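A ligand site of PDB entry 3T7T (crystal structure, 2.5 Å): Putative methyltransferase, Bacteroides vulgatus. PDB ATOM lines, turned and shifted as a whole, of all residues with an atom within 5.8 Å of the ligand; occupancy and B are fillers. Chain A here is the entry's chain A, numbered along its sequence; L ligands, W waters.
O of Gly 128 sits close to S1 of the ligand (3.5 Å).
Gly 33 touches the ligand.
Cys 61 touches the ligand (O to C1, 3.7 Å).
Phe 84 touches the ligand (CD1 to O5, 3.7 Å).
CD2 of Phe 87 touches O4 of the ligand (3.7 Å).
O of Gly 109 touches C13 of the ligand (3.7 Å).
CB of Ala 129 touches O3 of the ligand, 3.6 Å away.
Tyr 131 touches the ligand (OH to C5, 3.98 Å).
19 residues have an atom within 4 Å of the ligand: Arg 31, Gln 32, Gly 33, Gly 60, Cys 61, Gly 62, Gln 66, Asp 82, Phe 83, Phe 84, Phe 87, Gly 109, Ser 110, Met 111, Glu 127, Gly 128, Ala 129, Tyr 131 and Asn 132.
Water W4 lies within hydrogen-bond range of O of Pro 34 (2.9 Å), O1 of the ligand (2.9 Å), O of Glu 127 (3.4 Å) and N of Gly 128 (3.5 Å).
Water W3 lies within hydrogen-bond range of OG1 of Thr 63 (2.9 Å), N of Gly 65 (2.9 Å), O2 of the ligand (3.2 Å) and O of Glu 30 (3.3 Å).
The backbone NH (N) of Gln 32 lies within hydrogen-bond range of an oxygen (O2) of the ligand (3.3 Å).
The backbone NH (N) of Gly 62 sits close to an oxygen (O4) of the ligand (3.3 Å).
N4 of the ligand sits at hydrogen-bond distance from OG of Ser 110.
N of Phe 83 lies within hydrogen-bond range of N6 of the ligand (3.4 Å).
The backbone NH (N) of Met 111 sits at hydrogen-bond distance from a nitrogen (N5) of the ligand, at 3.0 Å.
The backbone carbonyl oxygen (O) of Gly 60 is in hydrogen-bond range of a nitrogen (N1) of the ligand.
An oxygen (O1) of the ligand lies close to the side-chain amide oxygen (OE1) of Gln 66 (3.1 Å).
N3 of the ligand sits close to OD1 of Asn 132 (3.2 Å).
NE2 of Gln 32 lies close to S1 of the ligand, 3.6 Å away.
OD1 of Asp 82 sits at hydrogen-bond distance from O4 of the ligand, 2.5 Å away.
An oxygen (O1) of the ligand is in salt-bridge range of the guanidinium group (NH1) of Arg 31 (2.9 Å).
The backbone carbonyl oxygen (O) of Glu 127 is in hydrogen-bond range of a nitrogen (N1) of the ligand (2.7 Å).
The side-chain carboxylate (OE1) of Glu 127 is in salt-bridge range of the guanidinium group (NH1) of Arg 31, at 2.9 Å.
N of Gly 109 lies within hydrogen-bond range of O of Asp 82.
OG of Ser 110 is in hydrogen-bond range of OD1 of Asp 112 (3.1 Å).
N of Cys 61 is in hydrogen-bond range of O of Ile 81 (3.3 Å).
N of Phe 84 lies within hydrogen-bond range of OD2 of Asp 82 (3.3 Å).
The side-chain amide nitrogen of Gln 66 sits at hydrogen-bond distance from the backbone carbonyl oxygen of Cys 61 (3.2 Å).
The backbone NH of Gly 60 is in hydrogen-bond range of the backbone carbonyl oxygen of Ile 81 (2.8 Å).
The backbone carbonyl oxygen (O) of Gly 109 sits at hydrogen-bond distance from the backbone NH (N) of Phe 83.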
ATOM      1  N   GLU A  30      22.459   7.937  10.365  1.00  0.00           N
ATOM      2  CA  GLU A  30      22.577   7.300   9.056  1.00  0.00           C
ATOM      3  C   GLU A  30      23.624   6.148   9.073  1.00  0.00           C
ATOM      4  O   GLU A  30      23.423   5.130   8.399  1.00  0.00           O
ATOM      5  CB  GLU A  30      23.000   8.356   8.004  1.00  0.00           C
ATOM      6  CG  GLU A  30      24.442   8.963   8.208  1.00  0.00           C
ATOM      7  CD  GLU A  30      24.902   9.927   7.082  1.00  0.00           C
ATOM      8  OE1 GLU A  30      24.565  11.132   7.120  1.00  0.00           O
ATOM      9  OE2 GLU A  30      25.614   9.463   6.152  1.00  0.00           O
ATOM     10  N   ARG A  31      24.718   6.321   9.824  1.00  0.00           N
ATOM     11  CA  ARG A  31      25.829   5.337   9.909  1.00  0.00           C
ATOM     12  C   ARG A  31      26.667   5.494  11.192  1.00  0.00           C
ATOM     13  O   ARG A  31      26.746   6.588  11.750  1.00  0.00           O
ATOM     14  CB  ARG A  31      26.745   5.507   8.687  1.00  0.00           C
ATOM     15  CG  ARG A  31      25.994   5.584   7.375  1.00  0.00           C
ATOM     16  CD  ARG A  31      26.895   5.511   6.162  1.00  0.00           C
ATOM     17  NE  ARG A  31      27.811   4.382   6.218  1.00  0.00           N
ATOM     18  CZ  ARG A  31      28.595   4.017   5.213  1.00  0.00           C
ATOM     19  NH1 ARG A  31      29.427   2.988   5.337  1.00  0.00           N
ATOM     20  NH2 ARG A  31      28.517   4.664   4.043  1.00  0.00           N
ATOM     21  N   GLN A  32      27.323   4.417  11.654  1.00  0.00           N
ATOM     22  CA  GLN A  32      28.160   4.526  12.863  1.00  0.00           C
ATOM     23  C   GLN A  32      29.625   4.797  12.572  1.00  0.00           C
ATOM     24  O   GLN A  32      30.430   4.916  13.503  1.00  0.00           O
ATOM     25  CB  GLN A  32      28.081   3.273  13.771  1.00  0.00           C
ATOM     26  CG  GLN A  32      28.989   3.405  15.065  1.00  0.00           C
ATOM     27  CD  GLN A  32      29.121   2.150  15.978  1.00  0.00           C
ATOM     28  OE1 GLN A  32      29.983   2.099  16.871  1.00  0.00           O
ATOM     29  NE2 GLN A  32      28.244   1.161  15.765  1.00  0.00           N
ATOM     30  N   GLY A  33      29.987   4.879  11.301  1.00  0.00           N
ATOM     31  CA  GLY A  33      31.370   5.134  10.951  1.00  0.00           C
ATOM     32  C   GLY A  33      31.524   5.957   9.695  1.00  0.00           C
ATOM     33  O   GLY A  33      30.564   6.116   8.943  1.00  0.00           O
ATOM     34  N   PRO A  34      32.719   6.503   9.441  1.00  0.00           N
ATOM     35  CA  PRO A  34      32.964   7.320   8.249  1.00  0.00           C
ATOM     36  C   PRO A  34      32.529   6.602   6.980  1.00  0.00           C
ATOM     37  O   PRO A  34      32.635   5.375   6.869  1.00  0.00           O
ATOM     38  CB  PRO A  34      34.476   7.534   8.275  1.00  0.00           C
ATOM     39  CG  PRO A  34      34.788   7.507   9.743  1.00  0.00           C
ATOM     40  CD  PRO A  34      33.936   6.358  10.254  1.00  0.00           C
ATOM     41  N   ASP A  58      27.790  -8.539   4.098  1.00  0.00           N
ATOM     42  CA  ASP A  58      28.279  -7.265   4.583  1.00  0.00           C
ATOM     43  C   ASP A  58      28.495  -7.504   6.075  1.00  0.00           C
ATOM     44  O   ASP A  58      27.524  -7.704   6.807  1.00  0.00           O
ATOM     45  CB  ASP A  58      27.222  -6.188   4.367  1.00  0.00           C
ATOM     46  CG  ASP A  58      27.672  -4.847   4.853  1.00  0.00           C
ATOM     47  OD1 ASP A  58      28.799  -4.741   5.372  1.00  0.00           O
ATOM     48  OD2 ASP A  58      26.895  -3.883   4.712  1.00  0.00           O
ATOM     49  N   LEU A  59      29.760  -7.492   6.485  1.00  0.00           N
ATOM     50  CA  LEU A  59      30.128  -7.746   7.884  1.00  0.00           C
ATOM     51  C   LEU A  59      30.246  -6.460   8.716  1.00  0.00           C
ATOM     52  O   LEU A  59      30.975  -5.524   8.363  1.00  0.00           O
ATOM     53  CB  LEU A  59      31.439  -8.555   7.934  1.00  0.00           C
ATOM     54  CG  LEU A  59      31.445  -9.849   7.098  1.00  0.00           C
ATOM     55  CD1 LEU A  59      32.694 -10.676   7.364  1.00  0.00           C
ATOM     56  CD2 LEU A  59      30.233 -10.662   7.436  1.00  0.00           C
ATOM     57  N   GLY A  60      29.518  -6.436   9.828  1.00  0.00           N
ATOM     58  CA  GLY A  60      29.531  -5.278  10.697  1.00  0.00           C
ATOM     59  C   GLY A  60      28.787  -4.180   9.961  1.00  0.00           C
ATOM     60  O   GLY A  60      29.269  -3.050   9.841  1.00  0.00           O
ATOM     61  N   CYS A  61      27.586  -4.540   9.500  1.00  0.00           N
ATOM     62  CA  CYS A  61      26.723  -3.667   8.723  1.00  0.00           C
ATOM     63  C   CYS A  61      26.025  -2.554   9.496  1.00  0.00           C
ATOM     64  O   CYS A  61      25.431  -1.669   8.870  1.00  0.00           O
ATOM     65  CB  CYS A  61      25.663  -4.500   7.988  1.00  0.00           C
ATOM     66  SG  CYS A  61      24.554  -5.478   9.054  1.00  0.00           S
ATOM     67  N   GLY A  62      26.109  -2.585  10.828  1.00  0.00           N
ATOM     68  CA  GLY A  62      25.434  -1.556  11.602  1.00  0.00           C
ATOM     69  C   GLY A  62      23.977  -1.515  11.167  1.00  0.00           C
ATOM     70  O   GLY A  62      23.363  -2.562  10.945  1.00  0.00           O
ATOM     71  N   THR A  63      23.415  -0.311  10.992  1.00  0.00           N
ATOM     72  CA  THR A  63      22.017  -0.188  10.584  1.00  0.00           C
ATOM     73  C   THR A  63      21.770  -0.600   9.135  1.00  0.00           C
ATOM     74  O   THR A  63      20.626  -0.690   8.693  1.00  0.00           O
ATOM     75  CB  THR A  63      21.482   1.247  10.817  1.00  0.00           C
ATOM     76  OG1 THR A  63      22.344   2.216  10.200  1.00  0.00           O
ATOM     77  CG2 THR A  63      21.385   1.526  12.313  1.00  0.00           C
ATOM     78  N   GLY A  65      23.039   1.023   6.369  1.00  0.00           N
ATOM     79  CA  GLY A  65      22.952   2.157   5.478  1.00  0.00           C
ATOM     80  C   GLY A  65      23.688   1.928   4.158  1.00  0.00           C
ATOM     81  O   GLY A  65      23.128   2.139   3.072  1.00  0.00           O
ATOM     82  N   GLN A  66      24.940   1.495   4.255  1.00  0.00           N
ATOM     83  CA  GLN A  66      25.721   1.237   3.064  1.00  0.00           C
ATOM     84  C   GLN A  66      25.184  -0.036   2.408  1.00  0.00           C
ATOM     85  O   GLN A  66      25.250  -0.197   1.187  1.00  0.00           O
ATOM     86  CB  GLN A  66      27.228   1.110   3.396  1.00  0.00           C
ATOM     87  CG  GLN A  66      27.692  -0.147   4.138  1.00  0.00           C
ATOM     88  CD  GLN A  66      27.290  -0.182   5.602  1.00  0.00           C
ATOM     89  OE1 GLN A  66      27.325   0.833   6.294  1.00  0.00           O
ATOM     90  NE2 GLN A  66      26.913  -1.365   6.081  1.00  0.00           N
ATOM     91  N   ILE A  81      25.438  -8.769   8.659  1.00  0.00           N
ATOM     92  CA  ILE A  81      25.701  -9.395   9.940  1.00  0.00           C
ATOM     93  C   ILE A  81      26.214  -8.378  10.954  1.00  0.00           C
ATOM     94  O   ILE A  81      27.148  -7.614  10.667  1.00  0.00           O
ATOM     95  CB  ILE A  81      26.743 -10.520   9.814  1.00  0.00           C
ATOM     96  CG1 ILE A  81      26.170 -11.634   8.936  1.00  0.00           C
ATOM     97  CG2 ILE A  81      27.147 -11.009  11.196  1.00  0.00           C
ATOM     98  CD1 ILE A  81      27.066 -12.852   8.789  1.00  0.00           C
ATOM     99  N   ASP A  82      25.608  -8.322  12.126  1.00  0.00           N
ATOM    100  CA  ASP A  82      26.091  -7.385  13.110  1.00  0.00           C
ATOM    101  C   ASP A  82      25.896  -7.928  14.510  1.00  0.00           C
ATOM    102  O   ASP A  82      24.979  -8.715  14.762  1.00  0.00           O
ATOM    103  CB  ASP A  82      25.381  -6.051  12.983  1.00  0.00           C
ATOM    104  CG  ASP A  82      26.210  -4.902  13.522  1.00  0.00           C
ATOM    105  OD1 ASP A  82      27.237  -4.558  12.881  1.00  0.00           O
ATOM    106  OD2 ASP A  82      25.845  -4.350  14.578  1.00  0.00           O
ATOM    107  N   PHE A  83      26.768  -7.499  15.408  1.00  0.00           N
ATOM    108  CA  PHE A  83      26.711  -7.946  16.792  1.00  0.00           C
ATOM    109  C   PHE A  83      25.528  -7.377  17.574  1.00  0.00           C
ATOM    110  O   PHE A  83      24.920  -8.093  18.366  1.00  0.00           O
ATOM    111  CB  PHE A  83      28.026  -7.615  17.513  1.00  0.00           C
ATOM    112  CG  PHE A  83      28.244  -8.442  18.762  1.00  0.00           C
ATOM    113  CD1 PHE A  83      28.299  -9.838  18.671  1.00  0.00           C
ATOM    114  CD2 PHE A  83      28.329  -7.838  20.010  1.00  0.00           C
ATOM    115  CE1 PHE A  83      28.423 -10.629  19.815  1.00  0.00           C
ATOM    116  CE2 PHE A  83      28.458  -8.621  21.164  1.00  0.00           C
ATOM    117  CZ  PHE A  83      28.505 -10.016  21.066  1.00  0.00           C
ATOM    118  N   PHE A  84      25.196  -6.099  17.357  1.00  0.00           N
ATOM    119  CA  PHE A  84      24.075  -5.468  18.057  1.00  0.00           C
ATOM    120  C   PHE A  84      22.697  -5.825  17.464  1.00  0.00           C
ATOM    121  O   PHE A  84      22.416  -5.487  16.313  1.00  0.00           O
ATOM    122  CB  PHE A  84      24.223  -3.936  18.049  1.00  0.00           C
ATOM    123  CG  PHE A  84      25.322  -3.388  18.955  1.00  0.00           C
ATOM    124  CD1 PHE A  84      26.477  -4.124  19.223  1.00  0.00           C
ATOM    125  CD2 PHE A  84      25.225  -2.082  19.460  1.00  0.00           C
ATOM    126  CE1 PHE A  84      27.522  -3.556  19.965  1.00  0.00           C
ATOM    127  CE2 PHE A  84      26.273  -1.501  20.200  1.00  0.00           C
ATOM    128  CZ  PHE A  84      27.414  -2.236  20.454  1.00  0.00           C
ATOM    129  N   PHE A  87      20.707  -2.979  15.834  1.00  0.00           N
ATOM    130  CA  PHE A  87      21.006  -2.573  14.466  1.00  0.00           C
ATOM    131  C   PHE A  87      20.354  -3.501  13.444  1.00  0.00           C
ATOM    132  O   PHE A  87      19.879  -3.057  12.405  1.00  0.00           O
ATOM    133  CB  PHE A  87      22.509  -2.533  14.228  1.00  0.00           C
ATOM    134  CG  PHE A  87      23.228  -1.497  15.019  1.00  0.00           C
ATOM    135  CD1 PHE A  87      22.626  -0.274  15.302  1.00  0.00           C
ATOM    136  CD2 PHE A  87      24.527  -1.725  15.472  1.00  0.00           C
ATOM    137  CE1 PHE A  87      23.298   0.714  16.008  1.00  0.00           C
ATOM    138  CE2 PHE A  87      25.219  -0.733  16.185  1.00  0.00           C
ATOM    139  CZ  PHE A  87      24.606   0.482  16.451  1.00  0.00           C
ATOM    140  N   GLY A 109      25.071 -11.714  14.281  1.00  0.00           N
ATOM    141  CA  GLY A 109      26.173 -12.637  14.378  1.00  0.00           C
ATOM    142  C   GLY A 109      27.475 -11.927  14.695  1.00  0.00           C
ATOM    143  O   GLY A 109      27.461 -10.747  15.062  1.00  0.00           O
ATOM    144  N   SER A 110      28.595 -12.630  14.558  1.00  0.00           N
ATOM    145  CA  SER A 110      29.902 -12.051  14.835  1.00  0.00           C
ATOM    146  C   SER A 110      30.859 -12.425  13.714  1.00  0.00           C
ATOM    147  O   SER A 110      30.812 -13.549  13.224  1.00  0.00           O
ATOM    148  CB  SER A 110      30.446 -12.568  16.166  1.00  0.00           C
ATOM    149  OG  SER A 110      31.679 -11.954  16.483  1.00  0.00           O
ATOM    150  N   MET A 111      31.726 -11.491  13.328  1.00  0.00           N
ATOM    151  CA  MET A 111      32.706 -11.687  12.247  1.00  0.00           C
ATOM    152  C   MET A 111      33.722 -12.763  12.552  1.00  0.00           C
ATOM    153  O   MET A 111      34.325 -13.321  11.635  1.00  0.00           O
ATOM    154  CB  MET A 111      33.497 -10.417  11.955  1.00  0.00           C
ATOM    155  CG  MET A 111      32.891  -9.116  12.395  1.00  0.00           C
ATOM    156  SD  MET A 111      34.159  -7.848  12.308  1.00  0.00           S
ATOM    157  CE  MET A 111      34.920  -8.208  13.762  1.00  0.00           C
ATOM    158  N   ASP A 112      33.949 -13.032  13.838  1.00  0.00           N
ATOM    159  CA  ASP A 112      34.926 -14.051  14.218  1.00  0.00           C
ATOM    160  C   ASP A 112      34.343 -15.459  14.351  1.00  0.00           C
ATOM    161  O   ASP A 112      35.077 -16.420  14.599  1.00  0.00           O
ATOM    162  CB  ASP A 112      35.645 -13.635  15.521  1.00  0.00           C
ATOM    163  CG  ASP A 112      34.673 -13.343  16.657  1.00  0.00           C
ATOM    164  OD1 ASP A 112      33.754 -14.159  16.866  1.00  0.00           O
ATOM    165  OD2 ASP A 112      34.844 -12.305  17.335  1.00  0.00           O
ATOM    166  N   SER A 126      32.583  -4.640   4.060  1.00  0.00           N
ATOM    167  CA  SER A 126      32.746  -4.259   5.453  1.00  0.00           C
ATOM    168  C   SER A 126      33.330  -2.877   5.555  1.00  0.00           C
ATOM    169  O   SER A 126      34.507  -2.667   5.280  1.00  0.00           O
ATOM    170  CB  SER A 126      33.626  -5.239   6.222  1.00  0.00           C
ATOM    171  OG  SER A 126      33.496  -5.027   7.633  1.00  0.00           O
ATOM    172  N   GLU A 127      32.495  -1.932   5.967  1.00  0.00           N
ATOM    173  CA  GLU A 127      32.948  -0.567   6.123  1.00  0.00           C
ATOM    174  C   GLU A 127      33.100  -0.223   7.587  1.00  0.00           C
ATOM    175  O   GLU A 127      32.156  -0.340   8.365  1.00  0.00           O
ATOM    176  CB  GLU A 127      31.975   0.388   5.455  1.00  0.00           C
ATOM    177  CG  GLU A 127      31.897   0.174   3.975  1.00  0.00           C
ATOM    178  CD  GLU A 127      31.263   1.337   3.268  1.00  0.00           C
ATOM    179  OE1 GLU A 127      31.649   2.480   3.595  1.00  0.00           O
ATOM    180  OE2 GLU A 127      30.389   1.112   2.408  1.00  0.00           O
ATOM    181  N   GLY A 128      34.313   0.195   7.932  1.00  0.00           N
ATOM    182  CA  GLY A 128      34.635   0.598   9.285  1.00  0.00           C
ATOM    183  C   GLY A 128      34.155  -0.383  10.329  1.00  0.00           C
ATOM    184  O   GLY A 128      33.571   0.012  11.338  1.00  0.00           O
ATOM    185  N   ALA A 129      34.441  -1.657  10.092  1.00  0.00           N
ATOM    186  CA  ALA A 129      34.006  -2.687  11.026  1.00  0.00           C
ATOM    187  C   ALA A 129      35.037  -3.771  11.211  1.00  0.00           C
ATOM    188  O   ALA A 129      34.975  -4.512  12.189  1.00  0.00           O
ATOM    189  CB  ALA A 129      32.694  -3.297  10.559  1.00  0.00           C
ATOM    190  N   TYR A 131      38.015  -3.653  12.179  1.00  0.00           N
ATOM    191  CA  TYR A 131      38.925  -3.468  13.310  1.00  0.00           C
ATOM    192  C   TYR A 131      38.530  -4.309  14.502  1.00  0.00           C
ATOM    193  O   TYR A 131      39.360  -4.593  15.365  1.00  0.00           O
ATOM    194  CB  TYR A 131      38.966  -2.018  13.743  1.00  0.00           C
ATOM    195  CG  TYR A 131      37.656  -1.538  14.334  1.00  0.00           C
ATOM    196  CD1 TYR A 131      36.598  -1.170  13.502  1.00  0.00           C
ATOM    197  CD2 TYR A 131      37.482  -1.446  15.716  1.00  0.00           C
ATOM    198  CE1 TYR A 131      35.395  -0.727  14.035  1.00  0.00           C
ATOM    199  CE2 TYR A 131      36.286  -1.003  16.256  1.00  0.00           C
ATOM    200  CZ  TYR A 131      35.245  -0.640  15.420  1.00  0.00           C
ATOM    201  OH  TYR A 131      34.058  -0.200  15.949  1.00  0.00           O
ATOM    202  N   ASN A 132      37.260  -4.697  14.576  1.00  0.00           N
ATOM    203  CA  ASN A 132      36.757  -5.522  15.695  1.00  0.00           C
ATOM    204  C   ASN A 132      37.465  -6.883  15.750  1.00  0.00           C
ATOM    205  O   ASN A 132      37.644  -7.447  16.827  1.00  0.00           O
ATOM    206  CB  ASN A 132      35.239  -5.752  15.571  1.00  0.00           C
ATOM    207  CG  ASN A 132      34.392  -4.495  15.828  1.00  0.00           C
ATOM    208  OD1 ASN A 132      34.251  -4.044  16.963  1.00  0.00           O
ATOM    209  ND2 ASN A 132      33.823  -3.937  14.764  1.00  0.00           N
HETATM  210  N1  LIG L   1      29.479  -0.701   8.662  1.00  0.00           N
HETATM  211  C1  LIG L   1      28.560   0.248   9.301  1.00  0.00           C
HETATM  212  C2  LIG L   1      28.790   0.272  10.816  1.00  0.00           C
HETATM  213  C3  LIG L   1      30.234   0.640  11.160  1.00  0.00           C
HETATM  214  S1  LIG L   1      30.533   0.737  12.957  1.00  0.00           S
HETATM  215  C4  LIG L   1      28.749   1.643   8.709  1.00  0.00           C
HETATM  216  O1  LIG L   1      29.754   1.814   7.968  1.00  0.00           O
HETATM  217  O2  LIG L   1      27.884   2.498   8.987  1.00  0.00           O
HETATM  218  C5  LIG L   1      31.153  -0.946  13.336  1.00  0.00           C
HETATM  219  C6  LIG L   1      30.086  -2.044  13.223  1.00  0.00           C
HETATM  220  O3  LIG L   1      30.692  -3.299  13.572  1.00  0.00           O
HETATM  221  C7  LIG L   1      28.981  -1.790  14.251  1.00  0.00           C
HETATM  222  O4  LIG L   1      27.717  -2.196  13.709  1.00  0.00           O
HETATM  223  C8  LIG L   1      29.383  -2.737  15.382  1.00  0.00           C
HETATM  224  O5  LIG L   1      28.211  -3.088  16.122  1.00  0.00           O
HETATM  225  C9  LIG L   1      29.811  -3.924  14.518  1.00  0.00           C
HETATM  226  N2  LIG L   1      30.489  -5.008  15.268  1.00  0.00           N
HETATM  227  C10 LIG L   1      31.289  -4.867  16.325  1.00  0.00           C
HETATM  228  N3  LIG L   1      31.787  -6.054  16.661  1.00  0.00           N
HETATM  229  C11 LIG L   1      31.277  -6.978  15.854  1.00  0.00           C
HETATM  230  C12 LIG L   1      31.441  -8.339  15.703  1.00  0.00           C
HETATM  231  N4  LIG L   1      32.231  -9.038  16.522  1.00  0.00           N
HETATM  232  N5  LIG L   1      30.786  -8.977  14.709  1.00  0.00           N
HETATM  233  C13 LIG L   1      29.986  -8.311  13.901  1.00  0.00           C
HETATM  234  N6  LIG L   1      29.819  -7.001  14.008  1.00  0.00           N
HETATM  235  C14 LIG L   1      30.444  -6.298  14.963  1.00  0.00           C
HETATM  236  O   HOH W   1      29.942  -3.305   7.001  1.00  0.00           O
HETATM  237  O   HOH W   2      33.467  -8.351  19.123  1.00  0.00           O
HETATM  238  O   HOH W   3      24.720   2.099   8.525  1.00  0.00           O
HETATM  239  O   HOH W   4      32.373   3.038   8.535  1.00  0.00           O
